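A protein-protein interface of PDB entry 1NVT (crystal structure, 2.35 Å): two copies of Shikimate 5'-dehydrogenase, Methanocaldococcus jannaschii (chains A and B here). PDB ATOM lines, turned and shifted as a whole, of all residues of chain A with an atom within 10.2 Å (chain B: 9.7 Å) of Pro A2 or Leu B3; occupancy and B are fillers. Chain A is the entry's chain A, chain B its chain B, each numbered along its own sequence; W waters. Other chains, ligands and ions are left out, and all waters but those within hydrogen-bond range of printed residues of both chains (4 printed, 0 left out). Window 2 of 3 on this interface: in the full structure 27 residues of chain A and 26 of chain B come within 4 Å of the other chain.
Among the printed residues, pairs that only touch across the chains: Pro A2 with Leu B3 (3.5 Å), Leu A3 with Pro B2 (3.4 Å), Leu A3 with Leu B3 (3.7 Å), Gly A4 with Gly B4 (3.7 Å), Gly A4 with Ser B5 (3.2 Å), Gly A4 with Met B6 (3.9 Å), Ser A5 with Gly B4 (3.5 Å), Ser A5 with Ile B7 (3.8 Å), Met A6 with Leu B3 (3.98 Å), Ile A7 with Ser B5 (3.7 Å), Ile A7 with Ile B28 (3.6 Å), Ile A7 with Asn B31 (3.8 Å) and Asn A31 with Ile B7 (3.6 Å).
Hydrophobic or aromatic side chains of chain B that line the printed part of chain A: Pro B2, Leu B3, Met B6, Ile B7 and Ile B28.
Hydrophobic or aromatic side chains of chain A that line the printed part of chain B: Pro A2, Met A6 and Ile A7.
Water W3 lies within hydrogen-bond range of the backbone carbonyl oxygen (O) of Ile A7 (2.5 Å) and the side-chain amide nitrogen (ND2) of Asn B31 (2.8 Å).
Water W1 lies within hydrogen-bond range of O of Ile B7 and ND2 of Asn A31.
Water W4 lies within hydrogen-bond range of OG of Ser A5 (2.6 Å), O of Ser B5 (3.1 Å) and N of Ile B7 (3.5 Å).
Water W2 lies within hydrogen-bond range of OG of Ser B5, O of Ser A5 and N of Ile A7.
Pro A2 touches one residue of chain B.
Gly A4 touches just these residues of chain B: Gly B4 (3.7 Å), Ser B5 (3.2 Å) and Met B6 (3.9 Å).
Printed residues of chain B within 4 Å of Met A6: Leu B3 (3.98 Å) and Gly B4 (3.4 Å).
Printed residues of chain B within 4 Å of Asn A31: Ile B7 (3.6 Å).
Of the printed residues of chain A, Ser B5 touches Gly A4, Ser A5 and Ile A7.
The nearest residue of chain B that does not touch Pro A2 is Gly B4 (4.6 Å).
The nearest printed residue of chain A that does not touch Leu B3 is Gly A4 (5.5 Å).
Pro A2 touches Leu B3, and with the chains exchanged Leu A3 touches Pro B2.
Leu A3 touches Gly B4, but with the chains exchanged Gly A4 does not touch Leu B3 (5.5 Å).
Gly A4 touches Ser B5, and with the chains exchanged Ser A5 touches Gly B4.
Ser A5 touches Ile B7, and with the chains exchanged Ile A7 touches Ser B5.
Positions printed for both chains: 1, 2, 3, 4, 5, 6, 7, 31, 32, 33, 35 and 36.
Of the 16 pairs that touch across the chains among the printed residues, 13 have their exchanged pair printed and touching as well.
The side-chain amino group of Lys B35 sits at hydrogen-bond distance from the backbone carbonyl oxygen of Pro B2.
The side-chain amino group (NZ) of Lys B35 sits at hydrogen-bond distance from the backbone carbonyl oxygen (O) of Gly B4 (2.6 Å).
The backbone carbonyl oxygen of Ser A5 is in hydrogen-bond range of the backbone NH of Ser B5 (2.8 Å).
O of Leu A3 lies within hydrogen-bond range of N of Gly B4 (3.1 Å).
The side-chain sulfur (SD) of Met A6 lies close to the backbone NH (N) of Gly B4 (3.6 Å).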
ATOM      1  N   GLY A   1      -2.838  28.126  30.734  1.00  0.00           N
ATOM      2  CA  GLY A   1      -3.908  28.446  29.746  1.00  0.00           C
ATOM      3  C   GLY A   1      -3.953  27.495  28.559  1.00  0.00           C
ATOM      4  O   GLY A   1      -3.440  26.374  28.635  1.00  0.00           O
ATOM      5  N   PRO A   2      -4.563  27.917  27.439  1.00  0.00           N
ATOM      6  CA  PRO A   2      -4.681  27.101  26.224  1.00  0.00           C
ATOM      7  C   PRO A   2      -3.321  26.754  25.612  1.00  0.00           C
ATOM      8  O   PRO A   2      -2.310  27.405  25.904  1.00  0.00           O
ATOM      9  CB  PRO A   2      -5.494  27.991  25.279  1.00  0.00           C
ATOM     10  CG  PRO A   2      -6.234  28.920  26.206  1.00  0.00           C
ATOM     11  CD  PRO A   2      -5.206  29.230  27.251  1.00  0.00           C
ATOM     12  N   LEU A   3      -3.306  25.730  24.761  1.00  0.00           N
ATOM     13  CA  LEU A   3      -2.086  25.320  24.070  1.00  0.00           C
ATOM     14  C   LEU A   3      -2.040  26.046  22.727  1.00  0.00           C
ATOM     15  O   LEU A   3      -3.068  26.220  22.067  1.00  0.00           O
ATOM     16  CB  LEU A   3      -2.077  23.806  23.843  1.00  0.00           C
ATOM     17  CG  LEU A   3      -1.980  22.913  25.085  1.00  0.00           C
ATOM     18  CD1 LEU A   3      -1.911  21.450  24.649  1.00  0.00           C
ATOM     19  CD2 LEU A   3      -0.741  23.291  25.898  1.00  0.00           C
ATOM     20  N   GLY A   4      -0.850  26.468  22.314  1.00  0.00           N
ATOM     21  CA  GLY A   4      -0.741  27.186  21.058  1.00  0.00           C
ATOM     22  C   GLY A   4      -0.987  28.660  21.315  1.00  0.00           C
ATOM     23  O   GLY A   4      -1.710  29.024  22.244  1.00  0.00           O
ATOM     24  N   SER A   5      -0.394  29.506  20.481  1.00  0.00           N
ATOM     25  CA  SER A   5      -0.495  30.953  20.611  1.00  0.00           C
ATOM     26  C   SER A   5      -1.867  31.535  20.262  1.00  0.00           C
ATOM     27  O   SER A   5      -2.423  31.243  19.197  1.00  0.00           O
ATOM     28  CB  SER A   5       0.571  31.595  19.726  1.00  0.00           C
ATOM     29  OG  SER A   5       1.761  30.825  19.758  1.00  0.00           O
ATOM     30  N   MET A   6      -2.403  32.359  21.167  1.00  0.00           N
ATOM     31  CA  MET A   6      -3.705  33.010  20.964  1.00  0.00           C
ATOM     32  C   MET A   6      -3.434  34.321  20.234  1.00  0.00           C
ATOM     33  O   MET A   6      -3.270  35.370  20.859  1.00  0.00           O
ATOM     34  CB  MET A   6      -4.389  33.301  22.310  1.00  0.00           C
ATOM     35  CG  MET A   6      -4.607  32.077  23.199  1.00  0.00           C
ATOM     36  SD  MET A   6      -5.650  30.792  22.447  1.00  0.00           S
ATOM     37  CE  MET A   6      -7.198  31.691  22.245  1.00  0.00           C
ATOM     38  N   ILE A   7      -3.395  34.242  18.908  1.00  0.00           N
ATOM     39  CA  ILE A   7      -3.100  35.382  18.048  1.00  0.00           C
ATOM     40  C   ILE A   7      -4.260  36.319  17.742  1.00  0.00           C
ATOM     41  O   ILE A   7      -5.396  35.890  17.532  1.00  0.00           O
ATOM     42  CB  ILE A   7      -2.527  34.873  16.716  1.00  0.00           C
ATOM     43  CG1 ILE A   7      -1.293  34.024  17.003  1.00  0.00           C
ATOM     44  CG2 ILE A   7      -2.170  36.025  15.802  1.00  0.00           C
ATOM     45  CD1 ILE A   7      -1.094  32.960  15.992  1.00  0.00           C
ATOM     46  N   ASN A  31       7.560  30.073  21.954  1.00  0.00           N
ATOM     47  CA  ASN A  31       6.119  30.278  22.022  1.00  0.00           C
ATOM     48  C   ASN A  31       5.561  29.839  23.381  1.00  0.00           C
ATOM     49  O   ASN A  31       4.647  30.469  23.918  1.00  0.00           O
ATOM     50  CB  ASN A  31       5.411  29.561  20.864  1.00  0.00           C
ATOM     51  CG  ASN A  31       5.539  30.323  19.549  1.00  0.00           C
ATOM     52  OD1 ASN A  31       5.403  31.548  19.520  1.00  0.00           O
ATOM     53  ND2 ASN A  31       5.787  29.605  18.459  1.00  0.00           N
ATOM     54  N   ALA A  32       6.124  28.772  23.937  1.00  0.00           N
ATOM     55  CA  ALA A  32       5.711  28.278  25.248  1.00  0.00           C
ATOM     56  C   ALA A  32       6.085  29.308  26.312  1.00  0.00           C
ATOM     57  O   ALA A  32       5.341  29.532  27.264  1.00  0.00           O
ATOM     58  CB  ALA A  32       6.399  26.952  25.552  1.00  0.00           C
ATOM     59  N   ALA A  33       7.239  29.942  26.143  1.00  0.00           N
ATOM     60  CA  ALA A  33       7.698  30.935  27.102  1.00  0.00           C
ATOM     61  C   ALA A  33       6.889  32.219  27.011  1.00  0.00           C
ATOM     62  O   ALA A  33       6.763  32.950  27.998  1.00  0.00           O
ATOM     63  CB  ALA A  33       9.169  31.221  26.887  1.00  0.00           C
ATOM     64  N   PHE A  34       6.349  32.498  25.826  1.00  0.00           N
ATOM     65  CA  PHE A  34       5.527  33.692  25.631  1.00  0.00           C
ATOM     66  C   PHE A  34       4.204  33.471  26.359  1.00  0.00           C
ATOM     67  O   PHE A  34       3.755  34.326  27.129  1.00  0.00           O
ATOM     68  CB  PHE A  34       5.241  33.930  24.143  1.00  0.00           C
ATOM     69  CG  PHE A  34       6.415  34.463  23.362  1.00  0.00           C
ATOM     70  CD1 PHE A  34       6.601  34.090  22.035  1.00  0.00           C
ATOM     71  CD2 PHE A  34       7.313  35.354  23.936  1.00  0.00           C
ATOM     72  CE1 PHE A  34       7.666  34.595  21.291  1.00  0.00           C
ATOM     73  CE2 PHE A  34       8.381  35.866  23.202  1.00  0.00           C
ATOM     74  CZ  PHE A  34       8.559  35.484  21.874  1.00  0.00           C
ATOM     75  N   LYS A  35       3.581  32.320  26.113  1.00  0.00           N
ATOM     76  CA  LYS A  35       2.315  32.008  26.759  1.00  0.00           C
ATOM     77  C   LYS A  35       2.445  32.107  28.270  1.00  0.00           C
ATOM     78  O   LYS A  35       1.735  32.882  28.913  1.00  0.00           O
ATOM     79  CB  LYS A  35       1.843  30.602  26.398  1.00  0.00           C
ATOM     80  CG  LYS A  35       1.342  30.445  24.979  1.00  0.00           C
ATOM     81  CD  LYS A  35       0.177  29.458  24.930  1.00  0.00           C
ATOM     82  CE  LYS A  35      -1.148  30.138  25.286  1.00  0.00           C
ATOM     83  NZ  LYS A  35      -1.173  30.795  26.636  1.00  0.00           N
ATOM     84  N   ASP A  36       3.359  31.315  28.826  1.00  0.00           N
ATOM     85  CA  ASP A  36       3.605  31.284  30.265  1.00  0.00           C
ATOM     86  C   ASP A  36       3.617  32.679  30.888  1.00  0.00           C
ATOM     87  O   ASP A  36       2.926  32.920  31.880  1.00  0.00           O
ATOM     88  CB  ASP A  36       4.938  30.585  30.559  1.00  0.00           C
ATOM     89  CG  ASP A  36       5.147  30.331  32.044  1.00  0.00           C
ATOM     90  OD1 ASP A  36       4.409  29.497  32.616  1.00  0.00           O
ATOM     91  OD2 ASP A  36       6.044  30.969  32.638  1.00  0.00           O
ATOM     92  N   LYS A  37       4.400  33.589  30.307  1.00  0.00           N
ATOM     93  CA  LYS A  37       4.499  34.961  30.804  1.00  0.00           C
ATOM     94  C   LYS A  37       3.376  35.855  30.272  1.00  0.00           C
ATOM     95  O   LYS A  37       3.378  37.072  30.497  1.00  0.00           O
ATOM     96  CB  LYS A  37       5.861  35.562  30.428  1.00  0.00           C
ATOM     97  CG  LYS A  37       6.830  35.718  31.604  1.00  0.00           C
ATOM     98  CD  LYS A  37       7.048  34.406  32.343  1.00  0.00           C
ATOM     99  CE  LYS A  37       7.765  34.631  33.666  1.00  0.00           C
ATOM    100  NZ  LYS A  37       7.895  33.361  34.443  1.00  0.00           N
ATOM    101  N   GLY A  38       2.421  35.247  29.569  1.00  0.00           N
ATOM    102  CA  GLY A  38       1.296  35.993  29.019  1.00  0.00           C
ATOM    103  C   GLY A  38       1.651  37.120  28.060  1.00  0.00           C
ATOM    104  O   GLY A  38       0.940  38.128  27.988  1.00  0.00           O
ATOM    105  N   VAL A 276       9.832  25.847  31.553  1.00  0.00           N
ATOM    106  CA  VAL A 276       8.833  25.823  30.493  1.00  0.00           C
ATOM    107  C   VAL A 276       9.573  25.518  29.199  1.00  0.00           C
ATOM    108  O   VAL A 276       9.218  24.593  28.462  1.00  0.00           O
ATOM    109  CB  VAL A 276       8.116  27.182  30.364  1.00  0.00           C
ATOM    110  CG1 VAL A 276       7.166  27.160  29.182  1.00  0.00           C
ATOM    111  CG2 VAL A 276       7.351  27.483  31.641  1.00  0.00           C
ATOM    112  N   GLY B   1      -8.608  20.380  17.630  1.00  0.00           N
ATOM    113  CA  GLY B   1      -7.186  20.768  17.897  1.00  0.00           C
ATOM    114  C   GLY B   1      -7.037  21.716  19.075  1.00  0.00           C
ATOM    115  O   GLY B   1      -8.000  21.945  19.810  1.00  0.00           O
ATOM    116  N   PRO B   2      -5.834  22.281  19.292  1.00  0.00           N
ATOM    117  CA  PRO B   2      -5.588  23.213  20.403  1.00  0.00           C
ATOM    118  C   PRO B   2      -6.466  24.463  20.280  1.00  0.00           C
ATOM    119  O   PRO B   2      -7.005  24.742  19.208  1.00  0.00           O
ATOM    120  CB  PRO B   2      -4.101  23.545  20.256  1.00  0.00           C
ATOM    121  CG  PRO B   2      -3.535  22.313  19.591  1.00  0.00           C
ATOM    122  CD  PRO B   2      -4.587  21.999  18.557  1.00  0.00           C
ATOM    123  N   LEU B   3      -6.608  25.217  21.367  1.00  0.00           N
ATOM    124  CA  LEU B   3      -7.421  26.427  21.323  1.00  0.00           C
ATOM    125  C   LEU B   3      -6.707  27.499  20.476  1.00  0.00           C
ATOM    126  O   LEU B   3      -7.317  28.135  19.612  1.00  0.00           O
ATOM    127  CB  LEU B   3      -7.682  26.931  22.749  1.00  0.00           C
ATOM    128  CG  LEU B   3      -9.091  27.462  23.037  1.00  0.00           C
ATOM    129  CD1 LEU B   3     -10.130  26.438  22.592  1.00  0.00           C
ATOM    130  CD2 LEU B   3      -9.236  27.757  24.522  1.00  0.00           C
ATOM    131  N   GLY B   4      -5.413  27.683  20.723  1.00  0.00           N
ATOM    132  CA  GLY B   4      -4.641  28.652  19.965  1.00  0.00           C
ATOM    133  C   GLY B   4      -3.958  27.980  18.783  1.00  0.00           C
ATOM    134  O   GLY B   4      -4.224  26.812  18.488  1.00  0.00           O
ATOM    135  N   SER B   5      -3.075  28.708  18.104  1.00  0.00           N
ATOM    136  CA  SER B   5      -2.354  28.164  16.953  1.00  0.00           C
ATOM    137  C   SER B   5      -1.078  27.432  17.384  1.00  0.00           C
ATOM    138  O   SER B   5      -0.226  28.008  18.061  1.00  0.00           O
ATOM    139  CB  SER B   5      -1.989  29.296  15.978  1.00  0.00           C
ATOM    140  OG  SER B   5      -3.143  29.934  15.456  1.00  0.00           O
ATOM    141  N   MET B   6      -0.947  26.160  17.010  1.00  0.00           N
ATOM    142  CA  MET B   6       0.258  25.401  17.359  1.00  0.00           C
ATOM    143  C   MET B   6       1.320  25.635  16.279  1.00  0.00           C
ATOM    144  O   MET B   6       1.371  24.932  15.271  1.00  0.00           O
ATOM    145  CB  MET B   6      -0.052  23.902  17.485  1.00  0.00           C
ATOM    146  CG  MET B   6      -0.280  23.426  18.923  1.00  0.00           C
ATOM    147  SD  MET B   6       1.072  23.886  20.071  1.00  0.00           S
ATOM    148  CE  MET B   6       2.427  22.903  19.433  1.00  0.00           C
ATOM    149  N   ILE B   7       2.163  26.635  16.508  1.00  0.00           N
ATOM    150  CA  ILE B   7       3.214  27.000  15.572  1.00  0.00           C
ATOM    151  C   ILE B   7       4.435  26.104  15.702  1.00  0.00           C
ATOM    152  O   ILE B   7       4.799  25.697  16.803  1.00  0.00           O
ATOM    153  CB  ILE B   7       3.671  28.468  15.793  1.00  0.00           C
ATOM    154  CG1 ILE B   7       2.566  29.439  15.366  1.00  0.00           C
ATOM    155  CG2 ILE B   7       4.936  28.756  14.995  1.00  0.00           C
ATOM    156  CD1 ILE B   7       1.372  29.456  16.271  1.00  0.00           C
ATOM    157  N   ILE B  28      -8.327  36.838  13.360  1.00  0.00           N
ATOM    158  CA  ILE B  28      -9.263  35.961  14.058  1.00  0.00           C
ATOM    159  C   ILE B  28      -9.981  35.051  13.080  1.00  0.00           C
ATOM    160  O   ILE B  28     -10.092  33.837  13.298  1.00  0.00           O
ATOM    161  CB  ILE B  28     -10.315  36.785  14.815  1.00  0.00           C
ATOM    162  CG1 ILE B  28      -9.621  37.706  15.817  1.00  0.00           C
ATOM    163  CG2 ILE B  28     -11.274  35.863  15.555  1.00  0.00           C
ATOM    164  CD1 ILE B  28      -8.763  36.968  16.838  1.00  0.00           C
ATOM    165  N   ASN B  31      -7.160  32.560  11.246  1.00  0.00           N
ATOM    166  CA  ASN B  31      -6.515  31.534  12.048  1.00  0.00           C
ATOM    167  C   ASN B  31      -7.536  30.455  12.404  1.00  0.00           C
ATOM    168  O   ASN B  31      -7.219  29.272  12.449  1.00  0.00           O
ATOM    169  CB  ASN B  31      -5.912  32.149  13.302  1.00  0.00           C
ATOM    170  CG  ASN B  31      -4.644  32.921  13.003  1.00  0.00           C
ATOM    171  OD1 ASN B  31      -3.760  32.424  12.290  1.00  0.00           O
ATOM    172  ND2 ASN B  31      -4.533  34.132  13.555  1.00  0.00           N
ATOM    173  N   ALA B  32      -8.772  30.873  12.643  1.00  0.00           N
ATOM    174  CA  ALA B  32      -9.836  29.941  12.980  1.00  0.00           C
ATOM    175  C   ALA B  32     -10.048  28.985  11.820  1.00  0.00           C
ATOM    176  O   ALA B  32     -10.177  27.775  12.014  1.00  0.00           O
ATOM    177  CB  ALA B  32     -11.130  30.709  13.277  1.00  0.00           C
ATOM    178  N   ALA B  33     -10.061  29.524  10.604  1.00  0.00           N
ATOM    179  CA  ALA B  33     -10.258  28.701   9.423  1.00  0.00           C
ATOM    180  C   ALA B  33      -9.040  27.828   9.114  1.00  0.00           C
ATOM    181  O   ALA B  33      -9.188  26.719   8.609  1.00  0.00           O
ATOM    182  CB  ALA B  33     -10.606  29.573   8.233  1.00  0.00           C
ATOM    183  N   LYS B  35      -6.938  26.485  11.301  1.00  0.00           N
ATOM    184  CA  LYS B  35      -7.015  25.380  12.258  1.00  0.00           C
ATOM    185  C   LYS B  35      -8.093  24.355  11.927  1.00  0.00           C
ATOM    186  O   LYS B  35      -7.858  23.145  11.997  1.00  0.00           O
ATOM    187  CB  LYS B  35      -7.242  25.933  13.667  1.00  0.00           C
ATOM    188  CG  LYS B  35      -6.035  26.714  14.197  1.00  0.00           C
ATOM    189  CD  LYS B  35      -6.324  27.387  15.538  1.00  0.00           C
ATOM    190  CE  LYS B  35      -6.683  26.363  16.603  1.00  0.00           C
ATOM    191  NZ  LYS B  35      -5.584  25.362  16.804  1.00  0.00           N
ATOM    192  N   ASP B  36      -9.276  24.835  11.560  1.00  0.00           N
ATOM    193  CA  ASP B  36     -10.371  23.944  11.215  1.00  0.00           C
ATOM    194  C   ASP B  36      -9.998  23.011  10.053  1.00  0.00           C
ATOM    195  O   ASP B  36     -10.503  21.889   9.954  1.00  0.00           O
ATOM    196  CB  ASP B  36     -11.608  24.762  10.838  1.00  0.00           C
ATOM    197  CG  ASP B  36     -12.633  23.937  10.081  1.00  0.00           C
ATOM    198  OD1 ASP B  36     -12.836  24.199   8.871  1.00  0.00           O
ATOM    199  OD2 ASP B  36     -13.224  23.014  10.696  1.00  0.00           O
ATOM    200  N   ALA B 280     -16.284  32.910  14.456  1.00  0.00           N
ATOM    201  CA  ALA B 280     -15.054  33.338  15.115  1.00  0.00           C
ATOM    202  C   ALA B 280     -15.075  34.861  15.246  1.00  0.00           C
ATOM    203  O   ALA B 280     -14.675  35.414  16.271  1.00  0.00           O
ATOM    204  CB  ALA B 280     -13.845  32.889  14.313  1.00  0.00           C
ATOM    205  N   LYS B 284     -15.685  37.515  18.765  1.00  0.00           N
ATOM    206  CA  LYS B 284     -14.703  38.507  19.168  1.00  0.00           C
ATOM    207  C   LYS B 284     -15.334  39.895  19.156  1.00  0.00           C
ATOM    208  O   LYS B 284     -14.855  40.805  19.832  1.00  0.00           O
ATOM    209  CB  LYS B 284     -13.484  38.462  18.243  1.00  0.00           C
ATOM    210  CG  LYS B 284     -12.167  38.393  18.993  1.00  0.00           C
ATOM    211  CD  LYS B 284     -12.164  37.236  19.992  1.00  0.00           C
ATOM    212  CE  LYS B 284     -10.887  37.197  20.812  1.00  0.00           C
ATOM    213  NZ  LYS B 284      -9.683  36.913  19.972  1.00  0.00           N
HETATM  214  O   HOH W   1       4.701  26.692  19.205  1.00  0.00           O
HETATM  215  O   HOH W   2      -4.792  31.869  16.859  1.00  0.00           O
HETATM  216  O   HOH W   3      -6.133  34.221  15.791  1.00  0.00           O
HETATM  217  O   HOH W   4       2.440  28.273  19.544  1.00  0.00           O
